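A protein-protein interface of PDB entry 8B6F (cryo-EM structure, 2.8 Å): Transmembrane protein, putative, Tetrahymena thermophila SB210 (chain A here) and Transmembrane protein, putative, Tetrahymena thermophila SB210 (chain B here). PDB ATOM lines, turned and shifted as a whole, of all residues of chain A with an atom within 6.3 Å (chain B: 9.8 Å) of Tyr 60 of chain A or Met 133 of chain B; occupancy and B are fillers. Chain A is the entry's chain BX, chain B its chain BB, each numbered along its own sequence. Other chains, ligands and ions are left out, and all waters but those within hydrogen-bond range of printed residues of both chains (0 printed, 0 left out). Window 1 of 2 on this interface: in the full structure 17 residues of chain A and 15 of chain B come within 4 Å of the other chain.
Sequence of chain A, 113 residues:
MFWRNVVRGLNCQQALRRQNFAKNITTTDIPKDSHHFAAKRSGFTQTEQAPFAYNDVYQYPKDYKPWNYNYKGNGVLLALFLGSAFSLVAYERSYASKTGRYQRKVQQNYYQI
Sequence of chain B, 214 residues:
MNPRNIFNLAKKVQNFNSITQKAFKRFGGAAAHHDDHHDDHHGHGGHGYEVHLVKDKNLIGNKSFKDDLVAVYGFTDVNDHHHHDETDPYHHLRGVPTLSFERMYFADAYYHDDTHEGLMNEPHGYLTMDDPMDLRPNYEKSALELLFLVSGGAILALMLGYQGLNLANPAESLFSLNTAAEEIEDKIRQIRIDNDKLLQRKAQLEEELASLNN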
ATOM      1  N   ILE A  30      20.572   0.334 -37.872  1.00  0.00           N
ATOM      2  CA  ILE A  30      19.680   1.044 -36.950  1.00  0.00           C
ATOM      3  C   ILE A  30      18.768   0.035 -36.257  1.00  0.00           C
ATOM      4  O   ILE A  30      18.167  -0.814 -36.936  1.00  0.00           O
ATOM      5  CB  ILE A  30      18.857   2.090 -37.707  1.00  0.00           C
ATOM      6  CG1 ILE A  30      19.777   3.042 -38.480  1.00  0.00           C
ATOM      7  CG2 ILE A  30      17.977   2.872 -36.737  1.00  0.00           C
ATOM      8  CD1 ILE A  30      19.045   4.047 -39.347  1.00  0.00           C
ATOM      9  N   PRO A  31      18.639   0.070 -34.931  1.00  0.00           N
ATOM     10  CA  PRO A  31      17.615  -0.755 -34.279  1.00  0.00           C
ATOM     11  C   PRO A  31      16.232  -0.366 -34.774  1.00  0.00           C
ATOM     12  O   PRO A  31      15.935   0.814 -34.970  1.00  0.00           O
ATOM     13  CB  PRO A  31      17.792  -0.442 -32.789  1.00  0.00           C
ATOM     14  CG  PRO A  31      19.152   0.114 -32.668  1.00  0.00           C
ATOM     15  CD  PRO A  31      19.431   0.828 -33.950  1.00  0.00           C
ATOM     16  N   LYS A  32      15.377  -1.364 -34.967  1.00  0.00           N
ATOM     17  CA  LYS A  32      14.056  -1.091 -35.506  1.00  0.00           C
ATOM     18  C   LYS A  32      13.106  -2.215 -35.131  1.00  0.00           C
ATOM     19  O   LYS A  32      13.519  -3.340 -34.841  1.00  0.00           O
ATOM     20  CB  LYS A  32      14.100  -0.918 -37.027  1.00  0.00           C
ATOM     21  CG  LYS A  32      14.589  -2.148 -37.771  1.00  0.00           C
ATOM     22  CD  LYS A  32      14.531  -1.947 -39.274  1.00  0.00           C
ATOM     23  CE  LYS A  32      14.947  -3.207 -40.018  1.00  0.00           C
ATOM     24  NZ  LYS A  32      14.073  -4.371 -39.699  1.00  0.00           N
ATOM     25  N   TYR A  58      11.537   3.118 -34.382  1.00  0.00           N
ATOM     26  CA  TYR A  58      12.733   2.978 -33.565  1.00  0.00           C
ATOM     27  C   TYR A  58      12.447   2.095 -32.358  1.00  0.00           C
ATOM     28  O   TYR A  58      11.395   2.206 -31.723  1.00  0.00           O
ATOM     29  CB  TYR A  58      13.228   4.348 -33.101  1.00  0.00           C
ATOM     30  CG  TYR A  58      13.825   5.192 -34.202  1.00  0.00           C
ATOM     31  CD1 TYR A  58      15.129   4.988 -34.628  1.00  0.00           C
ATOM     32  CD2 TYR A  58      13.088   6.198 -34.807  1.00  0.00           C
ATOM     33  CE1 TYR A  58      15.681   5.759 -35.633  1.00  0.00           C
ATOM     34  CE2 TYR A  58      13.629   6.975 -35.812  1.00  0.00           C
ATOM     35  CZ  TYR A  58      14.926   6.752 -36.220  1.00  0.00           C
ATOM     36  OH  TYR A  58      15.467   7.522 -37.221  1.00  0.00           O
ATOM     37  N   GLN A  59      13.387   1.209 -32.047  1.00  0.00           N
ATOM     38  CA  GLN A  59      13.298   0.345 -30.877  1.00  0.00           C
ATOM     39  C   GLN A  59      14.505   0.611 -29.992  1.00  0.00           C
ATOM     40  O   GLN A  59      15.647   0.427 -30.424  1.00  0.00           O
ATOM     41  CB  GLN A  59      13.237  -1.129 -31.275  1.00  0.00           C
ATOM     42  CG  GLN A  59      12.979  -2.061 -30.106  1.00  0.00           C
ATOM     43  CD  GLN A  59      12.894  -3.510 -30.528  1.00  0.00           C
ATOM     44  OE1 GLN A  59      13.280  -3.868 -31.639  1.00  0.00           O
ATOM     45  NE2 GLN A  59      12.381  -4.354 -29.642  1.00  0.00           N
ATOM     46  N   TYR A  60      14.252   1.036 -28.766  1.00  0.00           N
ATOM     47  CA  TYR A  60      15.329   1.317 -27.835  1.00  0.00           C
ATOM     48  C   TYR A  60      15.766   0.042 -27.122  1.00  0.00           C
ATOM     49  O   TYR A  60      14.968  -0.881 -26.938  1.00  0.00           O
ATOM     50  CB  TYR A  60      14.886   2.352 -26.808  1.00  0.00           C
ATOM     51  CG  TYR A  60      14.788   3.751 -27.357  1.00  0.00           C
ATOM     52  CD1 TYR A  60      13.819   4.085 -28.291  1.00  0.00           C
ATOM     53  CD2 TYR A  60      15.660   4.743 -26.935  1.00  0.00           C
ATOM     54  CE1 TYR A  60      13.725   5.365 -28.793  1.00  0.00           C
ATOM     55  CE2 TYR A  60      15.576   6.025 -27.431  1.00  0.00           C
ATOM     56  CZ  TYR A  60      14.606   6.330 -28.360  1.00  0.00           C
ATOM     57  OH  TYR A  60      14.513   7.607 -28.857  1.00  0.00           O
ATOM     58  N   PRO A  61      17.029  -0.037 -26.710  1.00  0.00           N
ATOM     59  CA  PRO A  61      17.466  -1.201 -25.936  1.00  0.00           C
ATOM     60  C   PRO A  61      16.792  -1.223 -24.575  1.00  0.00           C
ATOM     61  O   PRO A  61      16.692  -0.198 -23.897  1.00  0.00           O
ATOM     62  CB  PRO A  61      18.980  -1.002 -25.812  1.00  0.00           C
ATOM     63  CG  PRO A  61      19.177   0.459 -25.952  1.00  0.00           C
ATOM     64  CD  PRO A  61      18.116   0.938 -26.898  1.00  0.00           C
ATOM     65  N   LYS A  62      16.328  -2.402 -24.180  1.00  0.00           N
ATOM     66  CA  LYS A  62      15.711  -2.543 -22.871  1.00  0.00           C
ATOM     67  C   LYS A  62      16.722  -2.198 -21.784  1.00  0.00           C
ATOM     68  O   LYS A  62      17.922  -2.454 -21.917  1.00  0.00           O
ATOM     69  CB  LYS A  62      15.185  -3.966 -22.678  1.00  0.00           C
ATOM     70  CG  LYS A  62      14.143  -4.390 -23.706  1.00  0.00           C
ATOM     71  CD  LYS A  62      12.871  -3.559 -23.596  1.00  0.00           C
ATOM     72  CE  LYS A  62      11.843  -3.965 -24.645  1.00  0.00           C
ATOM     73  NZ  LYS A  62      12.311  -3.692 -26.033  1.00  0.00           N
ATOM     74  N   TYR A  64      17.308   0.879 -21.017  1.00  0.00           N
ATOM     75  CA  TYR A  64      17.797   2.219 -21.310  1.00  0.00           C
ATOM     76  C   TYR A  64      16.953   3.242 -20.562  1.00  0.00           C
ATOM     77  O   TYR A  64      15.726   3.260 -20.689  1.00  0.00           O
ATOM     78  CB  TYR A  64      17.753   2.493 -22.813  1.00  0.00           C
ATOM     79  CG  TYR A  64      18.166   3.900 -23.182  1.00  0.00           C
ATOM     80  CD1 TYR A  64      19.501   4.221 -23.379  1.00  0.00           C
ATOM     81  CD2 TYR A  64      17.222   4.906 -23.331  1.00  0.00           C
ATOM     82  CE1 TYR A  64      19.884   5.505 -23.714  1.00  0.00           C
ATOM     83  CE2 TYR A  64      17.594   6.192 -23.666  1.00  0.00           C
ATOM     84  CZ  TYR A  64      18.926   6.485 -23.856  1.00  0.00           C
ATOM     85  OH  TYR A  64      19.303   7.764 -24.187  1.00  0.00           O
ATOM     86  N   PRO A  66      16.117   7.109 -20.087  1.00  0.00           N
ATOM     87  CA  PRO A  66      16.335   8.419 -20.724  1.00  0.00           C
ATOM     88  C   PRO A  66      16.708   9.531 -19.759  1.00  0.00           C
ATOM     89  O   PRO A  66      17.119  10.604 -20.221  1.00  0.00           O
ATOM     90  CB  PRO A  66      14.986   8.714 -21.397  1.00  0.00           C
ATOM     91  CG  PRO A  66      14.290   7.411 -21.479  1.00  0.00           C
ATOM     92  CD  PRO A  66      14.744   6.625 -20.298  1.00  0.00           C
ATOM     93  N   GLY B 125      11.404  11.103 -18.531  1.00  0.00           N
ATOM     94  CA  GLY B 125      11.845  12.310 -19.190  1.00  0.00           C
ATOM     95  C   GLY B 125      13.224  12.153 -19.807  1.00  0.00           C
ATOM     96  O   GLY B 125      14.003  11.263 -19.458  1.00  0.00           O
ATOM     97  N   TYR B 126      13.527  13.044 -20.745  1.00  0.00           N
ATOM     98  CA  TYR B 126      14.815  13.063 -21.426  1.00  0.00           C
ATOM     99  C   TYR B 126      15.714  14.082 -20.745  1.00  0.00           C
ATOM    100  O   TYR B 126      15.304  15.223 -20.514  1.00  0.00           O
ATOM    101  CB  TYR B 126      14.648  13.401 -22.907  1.00  0.00           C
ATOM    102  CG  TYR B 126      13.780  12.415 -23.651  1.00  0.00           C
ATOM    103  CD1 TYR B 126      14.241  11.138 -23.942  1.00  0.00           C
ATOM    104  CD2 TYR B 126      12.501  12.760 -24.061  1.00  0.00           C
ATOM    105  CE1 TYR B 126      13.452  10.233 -24.618  1.00  0.00           C
ATOM    106  CE2 TYR B 126      11.705  11.863 -24.738  1.00  0.00           C
ATOM    107  CZ  TYR B 126      12.186  10.600 -25.013  1.00  0.00           C
ATOM    108  OH  TYR B 126      11.394   9.704 -25.690  1.00  0.00           O
ATOM    109  N   MET B 129      18.055  17.738 -24.750  1.00  0.00           N
ATOM    110  CA  MET B 129      17.326  17.780 -26.009  1.00  0.00           C
ATOM    111  C   MET B 129      17.965  16.919 -27.092  1.00  0.00           C
ATOM    112  O   MET B 129      17.390  16.793 -28.176  1.00  0.00           O
ATOM    113  CB  MET B 129      17.222  19.227 -26.494  1.00  0.00           C
ATOM    114  CG  MET B 129      16.301  19.413 -27.682  1.00  0.00           C
ATOM    115  SD  MET B 129      15.795  21.127 -27.901  1.00  0.00           S
ATOM    116  CE  MET B 129      17.383  21.925 -28.095  1.00  0.00           C
ATOM    117  N   ASP B 130      19.128  16.326 -26.831  1.00  0.00           N
ATOM    118  CA  ASP B 130      19.771  15.476 -27.822  1.00  0.00           C
ATOM    119  C   ASP B 130      18.981  14.188 -28.023  1.00  0.00           C
ATOM    120  O   ASP B 130      18.516  13.567 -27.065  1.00  0.00           O
ATOM    121  CB  ASP B 130      21.201  15.145 -27.396  1.00  0.00           C
ATOM    122  CG  ASP B 130      22.116  16.349 -27.452  1.00  0.00           C
ATOM    123  OD1 ASP B 130      21.601  17.481 -27.554  1.00  0.00           O
ATOM    124  OD2 ASP B 130      23.349  16.163 -27.411  1.00  0.00           O
ATOM    125  N   ASP B 131      18.845  13.784 -29.279  1.00  0.00           N
ATOM    126  CA  ASP B 131      18.106  12.569 -29.598  1.00  0.00           C
ATOM    127  C   ASP B 131      18.939  11.345 -29.227  1.00  0.00           C
ATOM    128  O   ASP B 131      20.083  11.224 -29.678  1.00  0.00           O
ATOM    129  CB  ASP B 131      17.758  12.547 -31.085  1.00  0.00           C
ATOM    130  CG  ASP B 131      16.830  11.405 -31.455  1.00  0.00           C
ATOM    131  OD1 ASP B 131      16.828  10.376 -30.750  1.00  0.00           O
ATOM    132  OD2 ASP B 131      16.103  11.536 -32.461  1.00  0.00           O
ATOM    133  N   PRO B 132      18.412  10.422 -28.415  1.00  0.00           N
ATOM    134  CA  PRO B 132      19.202   9.224 -28.086  1.00  0.00           C
ATOM    135  C   PRO B 132      19.639   8.436 -29.306  1.00  0.00           C
ATOM    136  O   PRO B 132      20.746   7.886 -29.319  1.00  0.00           O
ATOM    137  CB  PRO B 132      18.250   8.410 -27.201  1.00  0.00           C
ATOM    138  CG  PRO B 132      17.307   9.401 -26.640  1.00  0.00           C
ATOM    139  CD  PRO B 132      17.127  10.445 -27.696  1.00  0.00           C
ATOM    140  N   MET B 133      18.797   8.359 -30.330  1.00  0.00           N
ATOM    141  CA  MET B 133      19.105   7.644 -31.566  1.00  0.00           C
ATOM    142  C   MET B 133      19.225   8.687 -32.672  1.00  0.00           C
ATOM    143  O   MET B 133      18.265   8.965 -33.392  1.00  0.00           O
ATOM    144  CB  MET B 133      18.031   6.606 -31.881  1.00  0.00           C
ATOM    145  CG  MET B 133      17.725   5.675 -30.720  1.00  0.00           C
ATOM    146  SD  MET B 133      16.625   4.321 -31.165  1.00  0.00           S
ATOM    147  CE  MET B 133      17.678   3.382 -32.267  1.00  0.00           C
ATOM    148  N   ASP B 134      20.419   9.252 -32.811  1.00  0.00           N
ATOM    149  CA  ASP B 134      20.703  10.276 -33.805  1.00  0.00           C
ATOM    150  C   ASP B 134      21.790   9.763 -34.735  1.00  0.00           C
ATOM    151  O   ASP B 134      22.811   9.241 -34.273  1.00  0.00           O
ATOM    152  CB  ASP B 134      21.145  11.578 -33.134  1.00  0.00           C
ATOM    153  CG  ASP B 134      21.168  12.749 -34.093  1.00  0.00           C
ATOM    154  OD1 ASP B 134      20.744  12.576 -35.254  1.00  0.00           O
ATOM    155  OD2 ASP B 134      21.610  13.841 -33.685  1.00  0.00           O
ATOM    156  N   LEU B 135      21.571   9.909 -36.038  1.00  0.00           N
ATOM    157  CA  LEU B 135      22.513   9.426 -37.036  1.00  0.00           C
ATOM    158  C   LEU B 135      23.547  10.470 -37.434  1.00  0.00           C
ATOM    159  O   LEU B 135      24.423  10.169 -38.251  1.00  0.00           O
ATOM    160  CB  LEU B 135      21.761   8.946 -38.283  1.00  0.00           C
ATOM    161  CG  LEU B 135      20.717   7.831 -38.121  1.00  0.00           C
ATOM    162  CD1 LEU B 135      21.250   6.688 -37.264  1.00  0.00           C
ATOM    163  CD2 LEU B 135      19.399   8.352 -37.562  1.00  0.00           C
ATOM    164  N   ARG B 136      23.471  11.677 -36.885  1.00  0.00           N
ATOM    165  CA  ARG B 136      24.436  12.716 -37.220  1.00  0.00           C
ATOM    166  C   ARG B 136      25.761  12.455 -36.505  1.00  0.00           C
ATOM    167  O   ARG B 136      25.769  12.145 -35.312  1.00  0.00           O
ATOM    168  CB  ARG B 136      23.904  14.092 -36.830  1.00  0.00           C
ATOM    169  CG  ARG B 136      22.721  14.545 -37.656  1.00  0.00           C
ATOM    170  CD  ARG B 136      22.346  15.984 -37.361  1.00  0.00           C
ATOM    171  NE  ARG B 136      21.798  16.144 -36.021  1.00  0.00           N
ATOM    172  CZ  ARG B 136      21.339  17.288 -35.530  1.00  0.00           C
ATOM    173  NH1 ARG B 136      21.354  18.401 -36.243  1.00  0.00           N
ATOM    174  NH2 ARG B 136      20.851  17.313 -34.295  1.00  0.00           N
ATOM    175  N   PRO B 137      26.897  12.579 -37.198  1.00  0.00           N
ATOM    176  CA  PRO B 137      28.193  12.506 -36.500  1.00  0.00           C
ATOM    177  C   PRO B 137      28.532  13.813 -35.788  1.00  0.00           C
ATOM    178  O   PRO B 137      29.555  14.453 -36.042  1.00  0.00           O
ATOM    179  CB  PRO B 137      29.161  12.181 -37.645  1.00  0.00           C
ATOM    180  CG  PRO B 137      28.559  12.833 -38.827  1.00  0.00           C
ATOM    181  CD  PRO B 137      27.068  12.735 -38.654  1.00  0.00           C
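The side-chain carboxylate of Asp 131 of chain B is in hydrogen-bond range of the backbone NH of Met 133 of chain B (2.8 Å).
Printed residues of chain A that touch a printed residue of chain B: Pro 31, Tyr 58, Tyr 60, Tyr 64 and Pro 66.
Among the printed residues, no Asp or Glu carboxylate lies within 4 Å of a Lys or Arg side-chain nitrogen of the other chain.
The backbone carbonyl oxygen (O) of Gly 125 of chain B lies close to the backbone carbonyl oxygen (O) of Pro 66 of chain A (3.3 Å).
Ile 30 of chain A touches none of the printed residues of chain B.
Pro 31 of chain A touches just one residue of chain B: Met 133.
Tyr 60 of chain A touches two residues of chain B.
No residue of chain B comes within 4 Å of Pro 61 of chain A.
Lys 62 of chain A touches none of the printed residues of chain B.
Of the printed residues of chain B, Pro 66 of chain A touches Gly 125 (3.2 Å) and Tyr 126 (3.6 Å).
Of the printed residues of chain A, Pro 132 of chain B touches Tyr 60 and Tyr 64.
Of chain A, only Pro 31, Tyr 58 and Tyr 60 come within 4 Å of Met 133 of chain B.
The nearest residue of chain A that does not touch Met 133 of chain B is Gln 59 of chain A (4.03 Å).
Among the printed residues, pairs that only touch across the chains: Tyr 64 of chain A with Pro 132 of chain B, Pro 31 of chain A with Met 133 of chain B, Pro 66 of chain A with Tyr 126 of chain B, Tyr 60 of chain A with Pro 132 of chain B, Tyr 58 of chain A with Met 133 of chain B and Tyr 60 of chain A with Met 133 of chain B.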
